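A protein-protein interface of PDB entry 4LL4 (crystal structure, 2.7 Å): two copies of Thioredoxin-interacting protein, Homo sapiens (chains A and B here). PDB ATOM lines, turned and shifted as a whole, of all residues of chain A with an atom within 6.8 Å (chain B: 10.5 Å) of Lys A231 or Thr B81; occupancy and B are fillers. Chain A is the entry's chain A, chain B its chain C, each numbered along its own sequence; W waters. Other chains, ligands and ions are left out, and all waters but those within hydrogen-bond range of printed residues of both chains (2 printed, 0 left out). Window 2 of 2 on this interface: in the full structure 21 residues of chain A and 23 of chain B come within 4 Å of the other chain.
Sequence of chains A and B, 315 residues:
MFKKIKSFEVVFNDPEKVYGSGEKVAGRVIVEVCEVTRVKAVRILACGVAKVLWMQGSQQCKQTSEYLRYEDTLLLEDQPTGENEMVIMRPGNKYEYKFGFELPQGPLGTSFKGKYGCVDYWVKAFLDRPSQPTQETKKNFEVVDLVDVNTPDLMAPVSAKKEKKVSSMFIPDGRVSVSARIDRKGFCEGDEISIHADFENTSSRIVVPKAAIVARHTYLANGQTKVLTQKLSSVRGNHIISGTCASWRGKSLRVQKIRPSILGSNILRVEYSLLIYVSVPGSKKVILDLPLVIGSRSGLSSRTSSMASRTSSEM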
ATOM      1  N   ALA A 211     -22.165  15.282 -15.355  1.00  0.00           N
ATOM      2  CA  ALA A 211     -22.539  16.246 -16.408  1.00  0.00           C
ATOM      3  C   ALA A 211     -21.399  16.383 -17.381  1.00  0.00           C
ATOM      4  O   ALA A 211     -20.185  16.216 -17.010  1.00  0.00           O
ATOM      5  CB  ALA A 211     -22.850  17.582 -15.813  1.00  0.00           C
ATOM      6  N   ALA A 212     -21.753  16.676 -18.629  1.00  0.00           N
ATOM      7  CA  ALA A 212     -20.689  16.947 -19.595  1.00  0.00           C
ATOM      8  C   ALA A 212     -21.216  17.811 -20.626  1.00  0.00           C
ATOM      9  O   ALA A 212     -22.437  17.777 -20.895  1.00  0.00           O
ATOM     10  CB  ALA A 212     -20.101  15.681 -20.237  1.00  0.00           C
ATOM     11  N   ILE A 213     -20.301  18.626 -21.164  1.00  0.00           N
ATOM     12  CA  ILE A 213     -20.596  19.437 -22.336  1.00  0.00           C
ATOM     13  C   ILE A 213     -20.095  18.594 -23.500  1.00  0.00           C
ATOM     14  O   ILE A 213     -18.946  18.150 -23.532  1.00  0.00           O
ATOM     15  CB  ILE A 213     -19.890  20.853 -22.273  1.00  0.00           C
ATOM     16  CG1 ILE A 213     -20.659  21.833 -21.390  1.00  0.00           C
ATOM     17  CG2 ILE A 213     -19.727  21.451 -23.657  1.00  0.00           C
ATOM     18  CD1 ILE A 213     -19.842  23.087 -21.003  1.00  0.00           C
ATOM     19  N   VAL A 214     -20.954  18.361 -24.456  1.00  0.00           N
ATOM     20  CA  VAL A 214     -20.505  17.598 -25.600  1.00  0.00           C
ATOM     21  C   VAL A 214     -20.587  18.408 -26.906  1.00  0.00           C
ATOM     22  O   VAL A 214     -21.360  19.360 -27.041  1.00  0.00           O
ATOM     23  CB  VAL A 214     -21.232  16.249 -25.694  1.00  0.00           C
ATOM     24  CG1 VAL A 214     -20.771  15.315 -24.532  1.00  0.00           C
ATOM     25  CG2 VAL A 214     -22.732  16.425 -25.641  1.00  0.00           C
ATOM     26  N   ALA A 215     -19.727  18.063 -27.845  1.00  0.00           N
ATOM     27  CA  ALA A 215     -19.615  18.824 -29.093  1.00  0.00           C
ATOM     28  C   ALA A 215     -19.904  17.817 -30.181  1.00  0.00           C
ATOM     29  O   ALA A 215     -19.247  16.738 -30.212  1.00  0.00           O
ATOM     30  CB  ALA A 215     -18.215  19.377 -29.228  1.00  0.00           C
ATOM     31  N   THR A 229     -18.851  13.002 -32.190  1.00  0.00           N
ATOM     32  CA  THR A 229     -19.072  13.486 -30.824  1.00  0.00           C
ATOM     33  C   THR A 229     -17.804  13.538 -29.947  1.00  0.00           C
ATOM     34  O   THR A 229     -17.127  12.527 -29.692  1.00  0.00           O
ATOM     35  CB  THR A 229     -20.104  12.635 -30.150  1.00  0.00           C
ATOM     36  OG1 THR A 229     -21.126  12.372 -31.102  1.00  0.00           O
ATOM     37  CG2 THR A 229     -20.734  13.356 -29.002  1.00  0.00           C
ATOM     38  N   GLN A 230     -17.518  14.741 -29.485  1.00  0.00           N
ATOM     39  CA  GLN A 230     -16.396  15.032 -28.628  1.00  0.00           C
ATOM     40  C   GLN A 230     -16.972  15.391 -27.246  1.00  0.00           C
ATOM     41  O   GLN A 230     -18.025  16.011 -27.143  1.00  0.00           O
ATOM     42  CB  GLN A 230     -15.653  16.230 -29.197  1.00  0.00           C
ATOM     43  CG  GLN A 230     -14.192  16.328 -28.863  1.00  0.00           C
ATOM     44  CD  GLN A 230     -13.578  17.775 -29.001  1.00  0.00           C
ATOM     45  OE1 GLN A 230     -13.942  18.575 -29.878  1.00  0.00           O
ATOM     46  NE2 GLN A 230     -12.625  18.082 -28.119  1.00  0.00           N
ATOM     47  N   LYS A 231     -16.297  14.940 -26.196  1.00  0.00           N
ATOM     48  CA  LYS A 231     -16.602  15.244 -24.815  1.00  0.00           C
ATOM     49  C   LYS A 231     -15.636  16.336 -24.353  1.00  0.00           C
ATOM     50  O   LYS A 231     -14.395  16.130 -24.383  1.00  0.00           O
ATOM     51  CB  LYS A 231     -16.372  13.977 -23.998  1.00  0.00           C
ATOM     52  CG  LYS A 231     -16.825  14.062 -22.542  1.00  0.00           C
ATOM     53  CD  LYS A 231     -16.132  12.941 -21.826  1.00  0.00           C
ATOM     54  CE  LYS A 231     -16.735  12.662 -20.490  1.00  0.00           C
ATOM     55  NZ  LYS A 231     -15.811  11.951 -19.532  1.00  0.00           N
ATOM     56  N   LEU A 232     -16.181  17.490 -23.954  1.00  0.00           N
ATOM     57  CA  LEU A 232     -15.347  18.586 -23.425  1.00  0.00           C
ATOM     58  C   LEU A 232     -15.309  18.540 -21.874  1.00  0.00           C
ATOM     59  O   LEU A 232     -14.986  17.510 -21.331  1.00  0.00           O
ATOM     60  CB  LEU A 232     -15.743  19.951 -24.004  1.00  0.00           C
ATOM     61  CG  LEU A 232     -15.834  20.074 -25.549  1.00  0.00           C
ATOM     62  CD1 LEU A 232     -16.319  21.451 -26.009  1.00  0.00           C
ATOM     63  CD2 LEU A 232     -14.525  19.814 -26.140  1.00  0.00           C
ATOM     64  N   SER A 233     -15.636  19.597 -21.141  1.00  0.00           N
ATOM     65  CA  SER A 233     -15.491  19.514 -19.677  1.00  0.00           C
ATOM     66  C   SER A 233     -16.513  18.601 -19.026  1.00  0.00           C
ATOM     67  O   SER A 233     -17.515  18.316 -19.592  1.00  0.00           O
ATOM     68  CB  SER A 233     -15.355  20.898 -18.992  1.00  0.00           C
ATOM     69  OG  SER A 233     -15.976  21.968 -19.705  1.00  0.00           O
ATOM     70  N   SER A 234     -16.211  18.080 -17.856  1.00  0.00           N
ATOM     71  CA  SER A 234     -17.160  17.231 -17.161  1.00  0.00           C
ATOM     72  C   SER A 234     -16.867  17.199 -15.697  1.00  0.00           C
ATOM     73  O   SER A 234     -15.743  17.446 -15.305  1.00  0.00           O
ATOM     74  CB  SER A 234     -17.179  15.804 -17.713  1.00  0.00           C
ATOM     75  OG  SER A 234     -16.033  15.062 -17.393  1.00  0.00           O
ATOM     76  N   GLN A 256     -14.867  25.467 -22.696  1.00  0.00           N
ATOM     77  CA  GLN A 256     -13.530  25.586 -23.317  1.00  0.00           C
ATOM     78  C   GLN A 256     -13.609  25.836 -24.833  1.00  0.00           C
ATOM     79  O   GLN A 256     -14.560  25.350 -25.506  1.00  0.00           O
ATOM     80  CB  GLN A 256     -12.667  24.377 -22.993  1.00  0.00           C
ATOM     81  CG  GLN A 256     -13.443  23.244 -22.354  1.00  0.00           C
ATOM     82  CD  GLN A 256     -12.609  22.014 -22.051  1.00  0.00           C
ATOM     83  OE1 GLN A 256     -11.772  22.000 -21.135  1.00  0.00           O
ATOM     84  NE2 GLN A 256     -12.860  20.958 -22.800  1.00  0.00           N
ATOM     85  N   LEU A 275     -25.180  17.732 -21.013  1.00  0.00           N
ATOM     86  CA  LEU A 275     -25.723  16.479 -20.607  1.00  0.00           C
ATOM     87  C   LEU A 275     -25.654  16.406 -19.116  1.00  0.00           C
ATOM     88  O   LEU A 275     -24.600  16.542 -18.535  1.00  0.00           O
ATOM     89  CB  LEU A 275     -24.898  15.337 -21.227  1.00  0.00           C
ATOM     90  CG  LEU A 275     -25.379  14.682 -22.557  1.00  0.00           C
ATOM     91  CD1 LEU A 275     -26.099  15.622 -23.514  1.00  0.00           C
ATOM     92  CD2 LEU A 275     -24.196  14.081 -23.253  1.00  0.00           C
ATOM     93  N   TYR A 277     -26.797  13.586 -16.358  1.00  0.00           N
ATOM     94  CA  TYR A 277     -27.215  12.205 -16.389  1.00  0.00           C
ATOM     95  C   TYR A 277     -26.968  11.546 -15.041  1.00  0.00           C
ATOM     96  O   TYR A 277     -26.233  12.028 -14.209  1.00  0.00           O
ATOM     97  CB  TYR A 277     -26.665  11.437 -17.638  1.00  0.00           C
ATOM     98  CG  TYR A 277     -25.118  11.355 -17.812  1.00  0.00           C
ATOM     99  CD1 TYR A 277     -24.344  12.503 -18.164  1.00  0.00           C
ATOM    100  CD2 TYR A 277     -24.421  10.116 -17.624  1.00  0.00           C
ATOM    101  CE1 TYR A 277     -22.915  12.407 -18.290  1.00  0.00           C
ATOM    102  CE2 TYR A 277     -23.046  10.026 -17.774  1.00  0.00           C
ATOM    103  CZ  TYR A 277     -22.292  11.164 -18.095  1.00  0.00           C
ATOM    104  OH  TYR A 277     -20.925  11.061 -18.202  1.00  0.00           O
ATOM    105  N   LYS A 285     -28.461   4.807 -18.479  1.00  0.00           N
ATOM    106  CA  LYS A 285     -28.440   6.136 -17.880  1.00  0.00           C
ATOM    107  C   LYS A 285     -29.833   6.791 -17.894  1.00  0.00           C
ATOM    108  O   LYS A 285     -30.715   6.388 -18.706  1.00  0.00           O
ATOM    109  CB  LYS A 285     -27.441   7.032 -18.613  1.00  0.00           C
ATOM    110  CG  LYS A 285     -26.020   6.512 -18.508  1.00  0.00           C
ATOM    111  CD  LYS A 285     -25.071   7.210 -19.485  1.00  0.00           C
ATOM    112  CE  LYS A 285     -23.657   6.728 -19.268  1.00  0.00           C
ATOM    113  NZ  LYS A 285     -23.196   5.563 -20.136  1.00  0.00           N
ATOM    114  N   LYS B  40     -13.810  -0.965 -27.396  1.00  0.00           N
ATOM    115  CA  LYS B  40     -13.223   0.306 -27.858  1.00  0.00           C
ATOM    116  C   LYS B  40     -14.059   1.042 -28.947  1.00  0.00           C
ATOM    117  O   LYS B  40     -14.124   2.284 -28.969  1.00  0.00           O
ATOM    118  CB  LYS B  40     -11.746   0.105 -28.281  1.00  0.00           C
ATOM    119  CG  LYS B  40     -11.097   1.297 -29.066  1.00  0.00           C
ATOM    120  CD  LYS B  40      -9.577   1.123 -29.346  1.00  0.00           C
ATOM    121  CE  LYS B  40      -8.691   1.695 -28.233  1.00  0.00           C
ATOM    122  NZ  LYS B  40      -7.259   1.266 -28.371  1.00  0.00           N
ATOM    123  N   LEU B  74     -20.305   3.480 -35.259  1.00  0.00           N
ATOM    124  CA  LEU B  74     -21.612   3.394 -34.626  1.00  0.00           C
ATOM    125  C   LEU B  74     -21.635   3.666 -33.128  1.00  0.00           C
ATOM    126  O   LEU B  74     -20.807   3.178 -32.367  1.00  0.00           O
ATOM    127  CB  LEU B  74     -22.186   2.029 -34.881  1.00  0.00           C
ATOM    128  CG  LEU B  74     -22.953   1.852 -36.181  1.00  0.00           C
ATOM    129  CD1 LEU B  74     -22.431   2.692 -37.359  1.00  0.00           C
ATOM    130  CD2 LEU B  74     -22.931   0.410 -36.459  1.00  0.00           C
ATOM    131  N   LEU B  75     -22.645   4.443 -32.741  1.00  0.00           N
ATOM    132  CA  LEU B  75     -22.908   4.886 -31.366  1.00  0.00           C
ATOM    133  C   LEU B  75     -24.152   4.249 -30.782  1.00  0.00           C
ATOM    134  O   LEU B  75     -25.167   4.233 -31.442  1.00  0.00           O
ATOM    135  CB  LEU B  75     -23.155   6.405 -31.375  1.00  0.00           C
ATOM    136  CG  LEU B  75     -22.011   7.307 -30.895  1.00  0.00           C
ATOM    137  CD1 LEU B  75     -22.591   8.592 -30.261  1.00  0.00           C
ATOM    138  CD2 LEU B  75     -21.107   6.536 -29.895  1.00  0.00           C
ATOM    139  N   LEU B  76     -24.096   3.766 -29.554  1.00  0.00           N
ATOM    140  CA  LEU B  76     -25.307   3.325 -28.870  1.00  0.00           C
ATOM    141  C   LEU B  76     -25.943   4.483 -28.146  1.00  0.00           C
ATOM    142  O   LEU B  76     -25.241   5.393 -27.645  1.00  0.00           O
ATOM    143  CB  LEU B  76     -25.032   2.217 -27.842  1.00  0.00           C
ATOM    144  CG  LEU B  76     -25.970   0.979 -27.756  1.00  0.00           C
ATOM    145  CD1 LEU B  76     -27.417   1.117 -28.419  1.00  0.00           C
ATOM    146  CD2 LEU B  76     -25.276  -0.280 -28.283  1.00  0.00           C
ATOM    147  N   GLU B  77     -27.273   4.439 -28.068  1.00  0.00           N
ATOM    148  CA  GLU B  77     -28.086   5.393 -27.289  1.00  0.00           C
ATOM    149  C   GLU B  77     -27.586   5.667 -25.847  1.00  0.00           C
ATOM    150  O   GLU B  77     -27.728   6.749 -25.327  1.00  0.00           O
ATOM    151  CB  GLU B  77     -29.472   4.827 -27.207  1.00  0.00           C
ATOM    152  CG  GLU B  77     -30.363   5.331 -28.252  1.00  0.00           C
ATOM    153  CD  GLU B  77     -31.693   5.712 -27.629  1.00  0.00           C
ATOM    154  OE1 GLU B  77     -32.508   4.775 -27.302  1.00  0.00           O
ATOM    155  OE2 GLU B  77     -31.898   6.948 -27.420  1.00  0.00           O
ATOM    156  N   ASP B  78     -27.011   4.660 -25.211  1.00  0.00           N
ATOM    157  CA  ASP B  78     -26.523   4.788 -23.852  1.00  0.00           C
ATOM    158  C   ASP B  78     -25.085   5.368 -23.777  1.00  0.00           C
ATOM    159  O   ASP B  78     -24.527   5.471 -22.697  1.00  0.00           O
ATOM    160  CB  ASP B  78     -26.596   3.414 -23.163  1.00  0.00           C
ATOM    161  CG  ASP B  78     -26.776   3.513 -21.642  1.00  0.00           C
ATOM    162  OD1 ASP B  78     -27.330   4.527 -21.131  1.00  0.00           O
ATOM    163  OD2 ASP B  78     -26.373   2.541 -20.952  1.00  0.00           O
ATOM    164  N   GLN B  79     -24.510   5.738 -24.931  1.00  0.00           N
ATOM    165  CA  GLN B  79     -23.150   6.335 -25.050  1.00  0.00           C
ATOM    166  C   GLN B  79     -23.258   7.829 -25.315  1.00  0.00           C
ATOM    167  O   GLN B  79     -22.815   8.280 -26.363  1.00  0.00           O
ATOM    168  CB  GLN B  79     -22.428   5.766 -26.296  1.00  0.00           C
ATOM    169  CG  GLN B  79     -21.762   4.374 -26.220  1.00  0.00           C
ATOM    170  CD  GLN B  79     -20.982   4.029 -27.544  1.00  0.00           C
ATOM    171  OE1 GLN B  79     -21.296   3.040 -28.241  1.00  0.00           O
ATOM    172  NE2 GLN B  79     -19.969   4.867 -27.883  1.00  0.00           N
ATOM    173  N   PRO B  80     -23.856   8.605 -24.419  1.00  0.00           N
ATOM    174  CA  PRO B  80     -24.139   9.956 -24.855  1.00  0.00           C
ATOM    175  C   PRO B  80     -22.899  10.869 -24.975  1.00  0.00           C
ATOM    176  O   PRO B  80     -22.940  11.889 -25.663  1.00  0.00           O
ATOM    177  CB  PRO B  80     -25.076  10.460 -23.781  1.00  0.00           C
ATOM    178  CG  PRO B  80     -24.660   9.746 -22.578  1.00  0.00           C
ATOM    179  CD  PRO B  80     -24.269   8.385 -23.031  1.00  0.00           C
ATOM    180  N   THR B  81     -21.801  10.472 -24.351  1.00  0.00           N
ATOM    181  CA  THR B  81     -20.541  11.206 -24.431  1.00  0.00           C
ATOM    182  C   THR B  81     -19.767  10.803 -25.663  1.00  0.00           C
ATOM    183  O   THR B  81     -18.592  11.107 -25.804  1.00  0.00           O
ATOM    184  CB  THR B  81     -19.696  10.941 -23.202  1.00  0.00           C
ATOM    185  OG1 THR B  81     -19.890   9.567 -22.824  1.00  0.00           O
ATOM    186  CG2 THR B  81     -20.148  11.863 -22.068  1.00  0.00           C
ATOM    187  N   GLY B  82     -20.439  10.103 -26.554  1.00  0.00           N
ATOM    188  CA  GLY B  82     -19.852   9.723 -27.815  1.00  0.00           C
ATOM    189  C   GLY B  82     -18.797   8.642 -27.760  1.00  0.00           C
ATOM    190  O   GLY B  82     -18.724   7.814 -26.829  1.00  0.00           O
ATOM    191  N   GLU B  83     -17.937   8.701 -28.768  1.00  0.00           N
ATOM    192  CA  GLU B  83     -17.203   7.533 -29.254  1.00  0.00           C
ATOM    193  C   GLU B  83     -15.717   7.452 -28.868  1.00  0.00           C
ATOM    194  O   GLU B  83     -15.108   6.370 -28.991  1.00  0.00           O
ATOM    195  CB  GLU B  83     -17.357   7.473 -30.780  1.00  0.00           C
ATOM    196  CG  GLU B  83     -16.983   8.812 -31.481  1.00  0.00           C
ATOM    197  CD  GLU B  83     -18.050   9.270 -32.444  1.00  0.00           C
ATOM    198  OE1 GLU B  83     -17.852   9.025 -33.647  1.00  0.00           O
ATOM    199  OE2 GLU B  83     -19.077   9.849 -32.004  1.00  0.00           O
ATOM    200  N   ASN B  84     -15.109   8.570 -28.435  1.00  0.00           N
ATOM    201  CA  ASN B  84     -13.816   8.418 -27.709  1.00  0.00           C
ATOM    202  C   ASN B  84     -14.028   7.961 -26.277  1.00  0.00           C
ATOM    203  O   ASN B  84     -13.107   8.018 -25.449  1.00  0.00           O
ATOM    204  CB  ASN B  84     -12.871   9.615 -27.823  1.00  0.00           C
ATOM    205  CG  ASN B  84     -11.631   9.293 -28.682  1.00  0.00           C
ATOM    206  OD1 ASN B  84     -10.943  10.203 -29.161  1.00  0.00           O
ATOM    207  ND2 ASN B  84     -11.347   7.997 -28.873  1.00  0.00           N
ATOM    208  N   GLU B  85     -15.250   7.457 -26.046  1.00  0.00           N
ATOM    209  CA  GLU B  85     -15.659   6.880 -24.794  1.00  0.00           C
ATOM    210  C   GLU B  85     -15.973   5.431 -25.069  1.00  0.00           C
ATOM    211  O   GLU B  85     -16.297   5.056 -26.209  1.00  0.00           O
ATOM    212  CB  GLU B  85     -16.885   7.610 -24.317  1.00  0.00           C
ATOM    213  CG  GLU B  85     -16.778   9.059 -24.664  1.00  0.00           C
ATOM    214  CD  GLU B  85     -15.982   9.825 -23.629  1.00  0.00           C
ATOM    215  OE1 GLU B  85     -16.651  10.293 -22.685  1.00  0.00           O
ATOM    216  OE2 GLU B  85     -14.726   9.956 -23.728  1.00  0.00           O
ATOM    217  N   MET B  86     -15.882   4.644 -24.004  1.00  0.00           N
ATOM    218  CA  MET B  86     -15.857   3.197 -24.076  1.00  0.00           C
ATOM    219  C   MET B  86     -16.980   2.538 -23.321  1.00  0.00           C
ATOM    220  O   MET B  86     -17.480   3.059 -22.322  1.00  0.00           O
ATOM    221  CB  MET B  86     -14.539   2.691 -23.520  1.00  0.00           C
ATOM    222  CG  MET B  86     -13.476   2.564 -24.580  1.00  0.00           C
ATOM    223  SD  MET B  86     -12.391   1.153 -24.251  1.00  0.00           S
ATOM    224  CE  MET B  86     -13.520  -0.034 -23.508  1.00  0.00           C
ATOM    225  N   VAL B  87     -17.326   1.352 -23.797  1.00  0.00           N
ATOM    226  CA  VAL B  87     -18.515   0.638 -23.365  1.00  0.00           C
ATOM    227  C   VAL B  87     -18.178  -0.646 -22.630  1.00  0.00           C
ATOM    228  O   VAL B  87     -17.010  -1.069 -22.606  1.00  0.00           O
ATOM    229  CB  VAL B  87     -19.436   0.338 -24.564  1.00  0.00           C
ATOM    230  CG1 VAL B  87     -18.676   0.503 -25.867  1.00  0.00           C
ATOM    231  CG2 VAL B  87     -20.068  -1.065 -24.459  1.00  0.00           C
ATOM    232  N   ILE B  88     -19.231  -1.266 -22.075  1.00  0.00           N
ATOM    233  CA  ILE B  88     -19.157  -2.269 -20.994  1.00  0.00           C
ATOM    234  C   ILE B  88     -20.258  -3.336 -21.153  1.00  0.00           C
ATOM    235  O   ILE B  88     -21.395  -3.140 -20.701  1.00  0.00           O
ATOM    236  CB  ILE B  88     -19.249  -1.559 -19.573  1.00  0.00           C
ATOM    237  CG1 ILE B  88     -17.845  -1.226 -19.000  1.00  0.00           C
ATOM    238  CG2 ILE B  88     -20.074  -2.387 -18.582  1.00  0.00           C
ATOM    239  CD1 ILE B  88     -17.101   0.013 -19.617  1.00  0.00           C
HETATM  240  O   HOH W   1     -21.242   7.041 -22.301  1.00  0.00           O
HETATM  241  O   HOH W   2     -24.617   2.878 -19.017  1.00  0.00           O
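The backbone NH of Leu A275 lies within hydrogen-bond range of the backbone carbonyl oxygen of Ala A212, at 2.7 Å.
The side-chain amide nitrogen (NE2) of Gln B79 sits at hydrogen-bond distance from the backbone carbonyl oxygen (O) of Gly B82 (3.4 Å).
The side-chain carboxylate of Glu B85 lies close to the side-chain hydroxyl of Thr B81 (3.3 Å).
OE2 of Glu B83 is in hydrogen-bond range of N of Thr A229 (3.2 Å).
NZ of Lys A231 lies within salt-bridge range of OE1 of Glu B85, 3.7 Å away.
The side-chain amino group of Lys A285 is in hydrogen-bond range of the backbone carbonyl oxygen of Asp B78, 2.9 Å away.
Of the 15 printed residues of chain A, 4 touch a printed residue of chain B.
Hydrophobic or aromatic side chains of chain A within 4 Å of the printed part of chain B: Leu A275.
Of the 16 printed residues of chain B, 6 touch a printed residue of chain A.
Hydrophobic or aromatic side chains of chain B within 4 Å of the printed part of chain A: Pro B80.
Among the printed residues, 7 pairs touch across the chains.
Among the printed residues, Asp or Glu carboxylates within 4 Å of a Lys or Arg side-chain nitrogen of the other chain: Lys A231 with Glu B85 (3.7 Å).
No residue of chain B comes within 4 Å of Ala A215.
Of the printed residues of chain B, Thr A229 touches Gly B82 (3.7 Å) and Glu B83 (3.2 Å).
No residue of chain B comes within 4 Å of Gln A230.
Lys A231 touches just these residues of chain B: Thr B81 and Glu B85.
No residue of chain B comes within 4 Å of Leu A232.
Printed residues of chain B within 4 Å of Lys A285: Asp B78 and Pro B80.
Glu B77 touches none of the printed residues of chain A.
Of the printed residues of chain A, Asp B78 touches Lys A285 (2.9 Å).
Of the printed residues of chain A, Thr B81 touches Lys A231 (3.8 Å).
Of the printed residues of chain A, Gly B82 touches Thr A229.
Asn B84 touches none of the printed residues of chain A.
No position is printed for both chains.
Of the 7 pairs that touch across the chains among the printed residues, none has its exchanged pair printed and touching as well.
Water W2 lies within hydrogen-bond range of the side-chain carboxylate of Asp B78 (2.6 Å) and the side-chain amino group of Lys A285 (3.2 Å).
Water W1 bridges the side-chain hydroxyl of Thr B81 and the side-chain amino group of Lys A285.
Among the printed residues, merely in contact across the chains: Leu A275 with Pro B80 (3.5 Å), Thr A229 with Gly B82 (3.7 Å), Lys A285 with Pro B80 (3.8 Å) and Lys A231 with Thr B81 (3.8 Å).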
